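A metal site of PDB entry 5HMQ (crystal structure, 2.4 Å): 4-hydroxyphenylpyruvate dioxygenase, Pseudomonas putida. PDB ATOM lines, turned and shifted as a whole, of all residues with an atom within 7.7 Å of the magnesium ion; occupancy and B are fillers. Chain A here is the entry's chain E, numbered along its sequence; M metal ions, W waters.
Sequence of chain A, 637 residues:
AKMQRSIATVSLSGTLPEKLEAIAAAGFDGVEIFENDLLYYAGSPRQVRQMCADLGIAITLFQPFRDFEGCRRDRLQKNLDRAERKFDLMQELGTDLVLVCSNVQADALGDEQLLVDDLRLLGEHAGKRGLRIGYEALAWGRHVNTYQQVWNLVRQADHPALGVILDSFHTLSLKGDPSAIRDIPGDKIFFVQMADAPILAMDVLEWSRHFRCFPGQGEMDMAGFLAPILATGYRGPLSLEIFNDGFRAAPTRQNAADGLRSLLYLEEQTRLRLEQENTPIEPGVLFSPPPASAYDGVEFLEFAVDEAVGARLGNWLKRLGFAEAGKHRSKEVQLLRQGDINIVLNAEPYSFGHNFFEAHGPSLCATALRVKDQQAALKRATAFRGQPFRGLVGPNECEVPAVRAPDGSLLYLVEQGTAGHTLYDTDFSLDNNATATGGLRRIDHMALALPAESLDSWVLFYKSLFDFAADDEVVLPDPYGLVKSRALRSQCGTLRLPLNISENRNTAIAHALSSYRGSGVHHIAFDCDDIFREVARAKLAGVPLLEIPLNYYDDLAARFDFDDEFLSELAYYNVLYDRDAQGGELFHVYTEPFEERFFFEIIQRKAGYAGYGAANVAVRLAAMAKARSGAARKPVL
Water W1 bridges NE2 of His 170 and OE1 of Glu 136.
The nearest printed residue that does not touch the magnesium ion is His 170 (4.03 Å).
The magnesium ion is bound by NE2 of Gln 193, OD2 of Asp 167, OE1 of Glu 241, OE2 of Glu 136, water W2 and water W1.
The guanidinium group (NH2) of Arg 212 lies within salt-bridge range of the side-chain carboxylate (OD1) of Asp 167, 3.4 Å away. The side-chain amide nitrogen (NE2) of Gln 63 lies within hydrogen-bond range of the side-chain carboxylate (OE2) of Glu 241. The backbone carbonyl oxygen of Glu 241 lies within hydrogen-bond range of the guanidinium group of Arg 212 (2.9 Å). The backbone carbonyl oxygen (O) of Met 194 lies within hydrogen-bond range of the backbone NH (N) of Glu 241 (3.3 Å). The side-chain amide oxygen (OE1) of Gln 193 sits close to the side-chain carboxylate (OE1) of Glu 32, at 3.1 Å. OD1 of Asp 167 sits at hydrogen-bond distance from N of His 170. The backbone carbonyl oxygen of Gln 193 sits at hydrogen-bond distance from the backbone NH of Ser 168 (2.9 Å). The side-chain carboxylate (OD1) of Asp 167 lies within hydrogen-bond range of the backbone NH (N) of Phe 169 (3.0 Å).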
ATOM      1  N   GLU A  32     -30.473  11.592  -4.756  1.00  0.00           N
ATOM      2  CA  GLU A  32     -30.770  12.647  -5.720  1.00  0.00           C
ATOM      3  C   GLU A  32     -30.501  12.099  -7.118  1.00  0.00           C
ATOM      4  O   GLU A  32     -29.383  11.691  -7.417  1.00  0.00           O
ATOM      5  CB  GLU A  32     -29.920  13.901  -5.485  1.00  0.00           C
ATOM      6  CG  GLU A  32     -29.485  14.172  -4.059  1.00  0.00           C
ATOM      7  CD  GLU A  32     -28.598  15.401  -3.982  1.00  0.00           C
ATOM      8  OE1 GLU A  32     -28.587  16.182  -4.965  1.00  0.00           O
ATOM      9  OE2 GLU A  32     -27.880  15.579  -2.979  1.00  0.00           O
ATOM     10  N   LEU A  61     -34.809  13.974  -4.489  1.00  0.00           N
ATOM     11  CA  LEU A  61     -34.596  15.192  -5.273  1.00  0.00           C
ATOM     12  C   LEU A  61     -34.325  14.815  -6.720  1.00  0.00           C
ATOM     13  O   LEU A  61     -33.670  13.801  -6.999  1.00  0.00           O
ATOM     14  CB  LEU A  61     -33.421  16.002  -4.707  1.00  0.00           C
ATOM     15  CG  LEU A  61     -32.993  17.245  -5.493  1.00  0.00           C
ATOM     16  CD1 LEU A  61     -34.075  18.302  -5.417  1.00  0.00           C
ATOM     17  CD2 LEU A  61     -31.679  17.793  -4.955  1.00  0.00           C
ATOM     18  N   GLN A  63     -32.585  16.705 -10.100  1.00  0.00           N
ATOM     19  CA  GLN A  63     -31.718  17.842 -10.383  1.00  0.00           C
ATOM     20  C   GLN A  63     -30.807  17.542 -11.581  1.00  0.00           C
ATOM     21  O   GLN A  63     -30.544  16.377 -11.884  1.00  0.00           O
ATOM     22  CB  GLN A  63     -30.873  18.188  -9.147  1.00  0.00           C
ATOM     23  CG  GLN A  63     -29.908  17.094  -8.727  1.00  0.00           C
ATOM     24  CD  GLN A  63     -28.475  17.574  -8.712  1.00  0.00           C
ATOM     25  OE1 GLN A  63     -28.045  18.323  -9.595  1.00  0.00           O
ATOM     26  NE2 GLN A  63     -27.710  17.157  -7.709  1.00  0.00           N
ATOM     27  N   LEU A  99     -34.370  20.735  -7.934  1.00  0.00           N
ATOM     28  CA  LEU A  99     -33.403  21.781  -7.638  1.00  0.00           C
ATOM     29  C   LEU A  99     -33.254  22.695  -8.857  1.00  0.00           C
ATOM     30  O   LEU A  99     -33.032  22.223  -9.971  1.00  0.00           O
ATOM     31  CB  LEU A  99     -32.047  21.164  -7.266  1.00  0.00           C
ATOM     32  CG  LEU A  99     -30.916  22.106  -6.831  1.00  0.00           C
ATOM     33  CD1 LEU A  99     -29.973  21.389  -5.889  1.00  0.00           C
ATOM     34  CD2 LEU A  99     -30.138  22.653  -8.032  1.00  0.00           C
ATOM     35  N   CYS A 101     -30.894  25.764 -10.006  1.00  0.00           N
ATOM     36  CA  CYS A 101     -29.675  26.509  -9.702  1.00  0.00           C
ATOM     37  C   CYS A 101     -29.666  27.848 -10.430  1.00  0.00           C
ATOM     38  O   CYS A 101     -30.154  27.968 -11.554  1.00  0.00           O
ATOM     39  CB  CYS A 101     -28.423  25.697 -10.063  1.00  0.00           C
ATOM     40  SG  CYS A 101     -28.426  24.955 -11.701  1.00  0.00           S
ATOM     41  N   GLU A 136     -31.256  27.042  -5.527  1.00  0.00           N
ATOM     42  CA  GLU A 136     -29.870  26.950  -5.068  1.00  0.00           C
ATOM     43  C   GLU A 136     -29.030  27.987  -5.798  1.00  0.00           C
ATOM     44  O   GLU A 136     -29.123  28.106  -7.022  1.00  0.00           O
ATOM     45  CB  GLU A 136     -29.296  25.545  -5.313  1.00  0.00           C
ATOM     46  CG  GLU A 136     -27.818  25.428  -4.987  1.00  0.00           C
ATOM     47  CD  GLU A 136     -27.161  24.226  -5.630  1.00  0.00           C
ATOM     48  OE1 GLU A 136     -27.288  24.066  -6.858  1.00  0.00           O
ATOM     49  OE2 GLU A 136     -26.506  23.434  -4.916  1.00  0.00           O
ATOM     50  N   ALA A 137     -28.207  28.716  -5.050  1.00  0.00           N
ATOM     51  CA  ALA A 137     -27.271  29.663  -5.636  1.00  0.00           C
ATOM     52  C   ALA A 137     -25.971  28.950  -5.983  1.00  0.00           C
ATOM     53  O   ALA A 137     -25.332  28.356  -5.100  1.00  0.00           O
ATOM     54  CB  ALA A 137     -27.004  30.827  -4.693  1.00  0.00           C
ATOM     55  N   LEU A 138     -25.574  29.020  -7.248  1.00  0.00           N
ATOM     56  CA  LEU A 138     -24.232  28.630  -7.623  1.00  0.00           C
ATOM     57  C   LEU A 138     -23.264  29.732  -7.220  1.00  0.00           C
ATOM     58  O   LEU A 138     -23.569  30.913  -7.368  1.00  0.00           O
ATOM     59  CB  LEU A 138     -24.140  28.378  -9.142  1.00  0.00           C
ATOM     60  CG  LEU A 138     -25.052  27.305  -9.718  1.00  0.00           C
ATOM     61  CD1 LEU A 138     -24.917  27.229 -11.238  1.00  0.00           C
ATOM     62  CD2 LEU A 138     -24.753  25.951  -9.092  1.00  0.00           C
ATOM     63  N   ILE A 165     -32.533  25.829  -1.093  1.00  0.00           N
ATOM     64  CA  ILE A 165     -31.623  24.698  -1.058  1.00  0.00           C
ATOM     65  C   ILE A 165     -30.225  25.215  -0.739  1.00  0.00           C
ATOM     66  O   ILE A 165     -29.766  26.173  -1.366  1.00  0.00           O
ATOM     67  CB  ILE A 165     -31.638  23.913  -2.383  1.00  0.00           C
ATOM     68  CG1 ILE A 165     -32.947  23.141  -2.521  1.00  0.00           C
ATOM     69  CG2 ILE A 165     -30.432  22.975  -2.463  1.00  0.00           C
ATOM     70  CD1 ILE A 165     -32.962  22.124  -3.651  1.00  0.00           C
ATOM     71  N   LEU A 166     -29.585  24.595   0.243  1.00  0.00           N
ATOM     72  CA  LEU A 166     -28.259  25.011   0.694  1.00  0.00           C
ATOM     73  C   LEU A 166     -27.212  23.995   0.268  1.00  0.00           C
ATOM     74  O   LEU A 166     -27.426  22.784   0.370  1.00  0.00           O
ATOM     75  CB  LEU A 166     -28.239  25.191   2.219  1.00  0.00           C
ATOM     76  CG  LEU A 166     -29.181  26.274   2.748  1.00  0.00           C
ATOM     77  CD1 LEU A 166     -29.275  26.229   4.257  1.00  0.00           C
ATOM     78  CD2 LEU A 166     -28.717  27.636   2.283  1.00  0.00           C
ATOM     79  N   ASP A 167     -26.069  24.501  -0.193  1.00  0.00           N
ATOM     80  CA  ASP A 167     -24.965  23.691  -0.689  1.00  0.00           C
ATOM     81  C   ASP A 167     -23.716  24.207  -0.001  1.00  0.00           C
ATOM     82  O   ASP A 167     -23.319  25.353  -0.218  1.00  0.00           O
ATOM     83  CB  ASP A 167     -24.854  23.797  -2.208  1.00  0.00           C
ATOM     84  CG  ASP A 167     -23.745  22.933  -2.806  1.00  0.00           C
ATOM     85  OD1 ASP A 167     -22.602  22.963  -2.303  1.00  0.00           O
ATOM     86  OD2 ASP A 167     -24.024  22.222  -3.798  1.00  0.00           O
ATOM     87  N   SER A 168     -23.100  23.361   0.833  1.00  0.00           N
ATOM     88  CA  SER A 168     -21.994  23.830   1.676  1.00  0.00           C
ATOM     89  C   SER A 168     -20.827  24.348   0.856  1.00  0.00           C
ATOM     90  O   SER A 168     -20.157  25.305   1.279  1.00  0.00           O
ATOM     91  CB  SER A 168     -21.540  22.723   2.623  1.00  0.00           C
ATOM     92  OG  SER A 168     -21.003  21.620   1.914  1.00  0.00           O
ATOM     93  N   PHE A 169     -20.557  23.769  -0.312  1.00  0.00           N
ATOM     94  CA  PHE A 169     -19.428  24.239  -1.096  1.00  0.00           C
ATOM     95  C   PHE A 169     -19.683  25.641  -1.635  1.00  0.00           C
ATOM     96  O   PHE A 169     -18.806  26.509  -1.568  1.00  0.00           O
ATOM     97  CB  PHE A 169     -19.087  23.296  -2.247  1.00  0.00           C
ATOM     98  CG  PHE A 169     -17.916  23.756  -3.068  1.00  0.00           C
ATOM     99  CD1 PHE A 169     -18.084  24.682  -4.092  1.00  0.00           C
ATOM    100  CD2 PHE A 169     -16.640  23.317  -2.785  1.00  0.00           C
ATOM    101  CE1 PHE A 169     -17.000  25.137  -4.816  1.00  0.00           C
ATOM    102  CE2 PHE A 169     -15.553  23.765  -3.514  1.00  0.00           C
ATOM    103  CZ  PHE A 169     -15.739  24.679  -4.530  1.00  0.00           C
ATOM    104  N   HIS A 170     -20.872  25.872  -2.193  1.00  0.00           N
ATOM    105  CA  HIS A 170     -21.155  27.180  -2.787  1.00  0.00           C
ATOM    106  C   HIS A 170     -21.061  28.301  -1.767  1.00  0.00           C
ATOM    107  O   HIS A 170     -20.650  29.422  -2.114  1.00  0.00           O
ATOM    108  CB  HIS A 170     -22.528  27.176  -3.451  1.00  0.00           C
ATOM    109  CG  HIS A 170     -22.610  26.340  -4.687  1.00  0.00           C
ATOM    110  ND1 HIS A 170     -21.761  26.516  -5.758  1.00  0.00           N
ATOM    111  CD2 HIS A 170     -23.451  25.340  -5.034  1.00  0.00           C
ATOM    112  CE1 HIS A 170     -22.066  25.650  -6.705  1.00  0.00           C
ATOM    113  NE2 HIS A 170     -23.095  24.917  -6.292  1.00  0.00           N
ATOM    114  N   VAL A 192     -30.538  20.069   1.727  1.00  0.00           N
ATOM    115  CA  VAL A 192     -29.180  20.414   2.157  1.00  0.00           C
ATOM    116  C   VAL A 192     -28.193  19.470   1.463  1.00  0.00           C
ATOM    117  O   VAL A 192     -28.312  18.241   1.589  1.00  0.00           O
ATOM    118  CB  VAL A 192     -29.019  20.329   3.684  1.00  0.00           C
ATOM    119  CG1 VAL A 192     -27.562  20.527   4.063  1.00  0.00           C
ATOM    120  CG2 VAL A 192     -29.900  21.363   4.366  1.00  0.00           C
ATOM    121  N   GLN A 193     -27.236  20.046   0.746  1.00  0.00           N
ATOM    122  CA  GLN A 193     -26.161  19.285   0.104  1.00  0.00           C
ATOM    123  C   GLN A 193     -24.860  19.578   0.824  1.00  0.00           C
ATOM    124  O   GLN A 193     -24.434  20.737   0.894  1.00  0.00           O
ATOM    125  CB  GLN A 193     -26.055  19.636  -1.377  1.00  0.00           C
ATOM    126  CG  GLN A 193     -27.279  19.301  -2.209  1.00  0.00           C
ATOM    127  CD  GLN A 193     -27.116  19.719  -3.654  1.00  0.00           C
ATOM    128  OE1 GLN A 193     -27.577  19.037  -4.577  1.00  0.00           O
ATOM    129  NE2 GLN A 193     -26.466  20.858  -3.870  1.00  0.00           N
ATOM    130  N   MET A 194     -24.230  18.540   1.359  1.00  0.00           N
ATOM    131  CA  MET A 194     -22.923  18.683   2.001  1.00  0.00           C
ATOM    132  C   MET A 194     -21.817  18.306   1.031  1.00  0.00           C
ATOM    133  O   MET A 194     -21.872  17.252   0.394  1.00  0.00           O
ATOM    134  CB  MET A 194     -22.830  17.821   3.262  1.00  0.00           C
ATOM    135  CG  MET A 194     -23.892  18.128   4.311  1.00  0.00           C
ATOM    136  SD  MET A 194     -23.877  19.991   4.892  1.00  0.00           S
ATOM    137  CE  MET A 194     -22.046  20.104   5.579  1.00  0.00           C
ATOM    138  N   ALA A 195     -20.820  19.167   0.910  1.00  0.00           N
ATOM    139  CA  ALA A 195     -19.685  18.918   0.024  1.00  0.00           C
ATOM    140  C   ALA A 195     -18.467  19.592   0.611  1.00  0.00           C
ATOM    141  O   ALA A 195     -18.490  20.807   0.863  1.00  0.00           O
ATOM    142  CB  ALA A 195     -19.960  19.437  -1.388  1.00  0.00           C
ATOM    143  N   SER A 208     -15.076  23.783  -7.827  1.00  0.00           N
ATOM    144  CA  SER A 208     -16.219  22.899  -7.549  1.00  0.00           C
ATOM    145  C   SER A 208     -16.208  21.683  -8.453  1.00  0.00           C
ATOM    146  O   SER A 208     -16.605  20.589  -8.028  1.00  0.00           O
ATOM    147  CB  SER A 208     -17.521  23.670  -7.724  1.00  0.00           C
ATOM    148  OG  SER A 208     -18.655  22.839  -7.544  1.00  0.00           O
ATOM    149  N   ARG A 212     -14.308  18.723  -5.142  1.00  0.00           N
ATOM    150  CA  ARG A 212     -15.278  18.387  -4.100  1.00  0.00           C
ATOM    151  C   ARG A 212     -14.981  16.995  -3.566  1.00  0.00           C
ATOM    152  O   ARG A 212     -14.592  16.085  -4.310  1.00  0.00           O
ATOM    153  CB  ARG A 212     -16.706  18.445  -4.648  1.00  0.00           C
ATOM    154  CG  ARG A 212     -17.328  19.825  -4.682  1.00  0.00           C
ATOM    155  CD  ARG A 212     -18.766  19.745  -5.159  1.00  0.00           C
ATOM    156  NE  ARG A 212     -19.369  21.049  -5.407  1.00  0.00           N
ATOM    157  CZ  ARG A 212     -20.615  21.364  -5.084  1.00  0.00           C
ATOM    158  NH1 ARG A 212     -21.385  20.465  -4.471  1.00  0.00           N
ATOM    159  NH2 ARG A 212     -21.088  22.575  -5.345  1.00  0.00           N
ATOM    160  N   LEU A 240     -25.350  14.565  -0.062  1.00  0.00           N
ATOM    161  CA  LEU A 240     -23.969  14.716  -0.494  1.00  0.00           C
ATOM    162  C   LEU A 240     -23.934  14.970  -1.990  1.00  0.00           C
ATOM    163  O   LEU A 240     -24.606  14.283  -2.757  1.00  0.00           O
ATOM    164  CB  LEU A 240     -23.175  13.444  -0.184  1.00  0.00           C
ATOM    165  CG  LEU A 240     -23.030  13.038   1.271  1.00  0.00           C
ATOM    166  CD1 LEU A 240     -22.561  11.589   1.376  1.00  0.00           C
ATOM    167  CD2 LEU A 240     -22.050  13.960   1.967  1.00  0.00           C
ATOM    168  N   GLU A 241     -23.139  15.966  -2.415  1.00  0.00           N
ATOM    169  CA  GLU A 241     -22.993  16.236  -3.845  1.00  0.00           C
ATOM    170  C   GLU A 241     -21.526  16.516  -4.168  1.00  0.00           C
ATOM    171  O   GLU A 241     -21.022  17.610  -3.901  1.00  0.00           O
ATOM    172  CB  GLU A 241     -23.882  17.400  -4.286  1.00  0.00           C
ATOM    173  CG  GLU A 241     -23.906  17.562  -5.797  1.00  0.00           C
ATOM    174  CD  GLU A 241     -24.547  18.863  -6.241  1.00  0.00           C
ATOM    175  OE1 GLU A 241     -24.393  19.879  -5.533  1.00  0.00           O
ATOM    176  OE2 GLU A 241     -25.217  18.858  -7.303  1.00  0.00           O
ATOM    177  N   ILE A 242     -20.855  15.521  -4.731  1.00  0.00           N
ATOM    178  CA  ILE A 242     -19.541  15.683  -5.339  1.00  0.00           C
ATOM    179  C   ILE A 242     -19.663  15.293  -6.800  1.00  0.00           C
ATOM    180  O   ILE A 242     -20.594  14.593  -7.199  1.00  0.00           O
ATOM    181  CB  ILE A 242     -18.432  14.873  -4.636  1.00  0.00           C
ATOM    182  CG1 ILE A 242     -18.638  13.366  -4.850  1.00  0.00           C
ATOM    183  CG2 ILE A 242     -18.389  15.202  -3.150  1.00  0.00           C
ATOM    184  CD1 ILE A 242     -17.519  12.522  -4.288  1.00  0.00           C
ATOM    185  N   PHE A 243     -18.754  15.812  -7.614  1.00  0.00           N
ATOM    186  CA  PHE A 243     -18.786  15.598  -9.057  1.00  0.00           C
ATOM    187  C   PHE A 243     -17.649  14.648  -9.438  1.00  0.00           C
ATOM    188  O   PHE A 243     -16.486  15.047  -9.478  1.00  0.00           O
ATOM    189  CB  PHE A 243     -18.674  16.919  -9.800  1.00  0.00           C
ATOM    190  CG  PHE A 243     -19.794  17.859  -9.504  1.00  0.00           C
ATOM    191  CD1 PHE A 243     -21.059  17.641 -10.030  1.00  0.00           C
ATOM    192  CD2 PHE A 243     -19.596  18.957  -8.681  1.00  0.00           C
ATOM    193  CE1 PHE A 243     -22.098  18.507  -9.753  1.00  0.00           C
ATOM    194  CE2 PHE A 243     -20.634  19.823  -8.403  1.00  0.00           C
ATOM    195  CZ  PHE A 243     -21.883  19.602  -8.934  1.00  0.00           C
HETATM  196 MG    MG M   1     -25.318  21.712  -5.276  1.00  0.00          MG
HETATM  197  O   HOH W   1     -24.457  22.679  -7.185  1.00  0.00           O
HETATM  198  O   HOH W   2     -26.692  20.974  -6.734  1.00  0.00           O
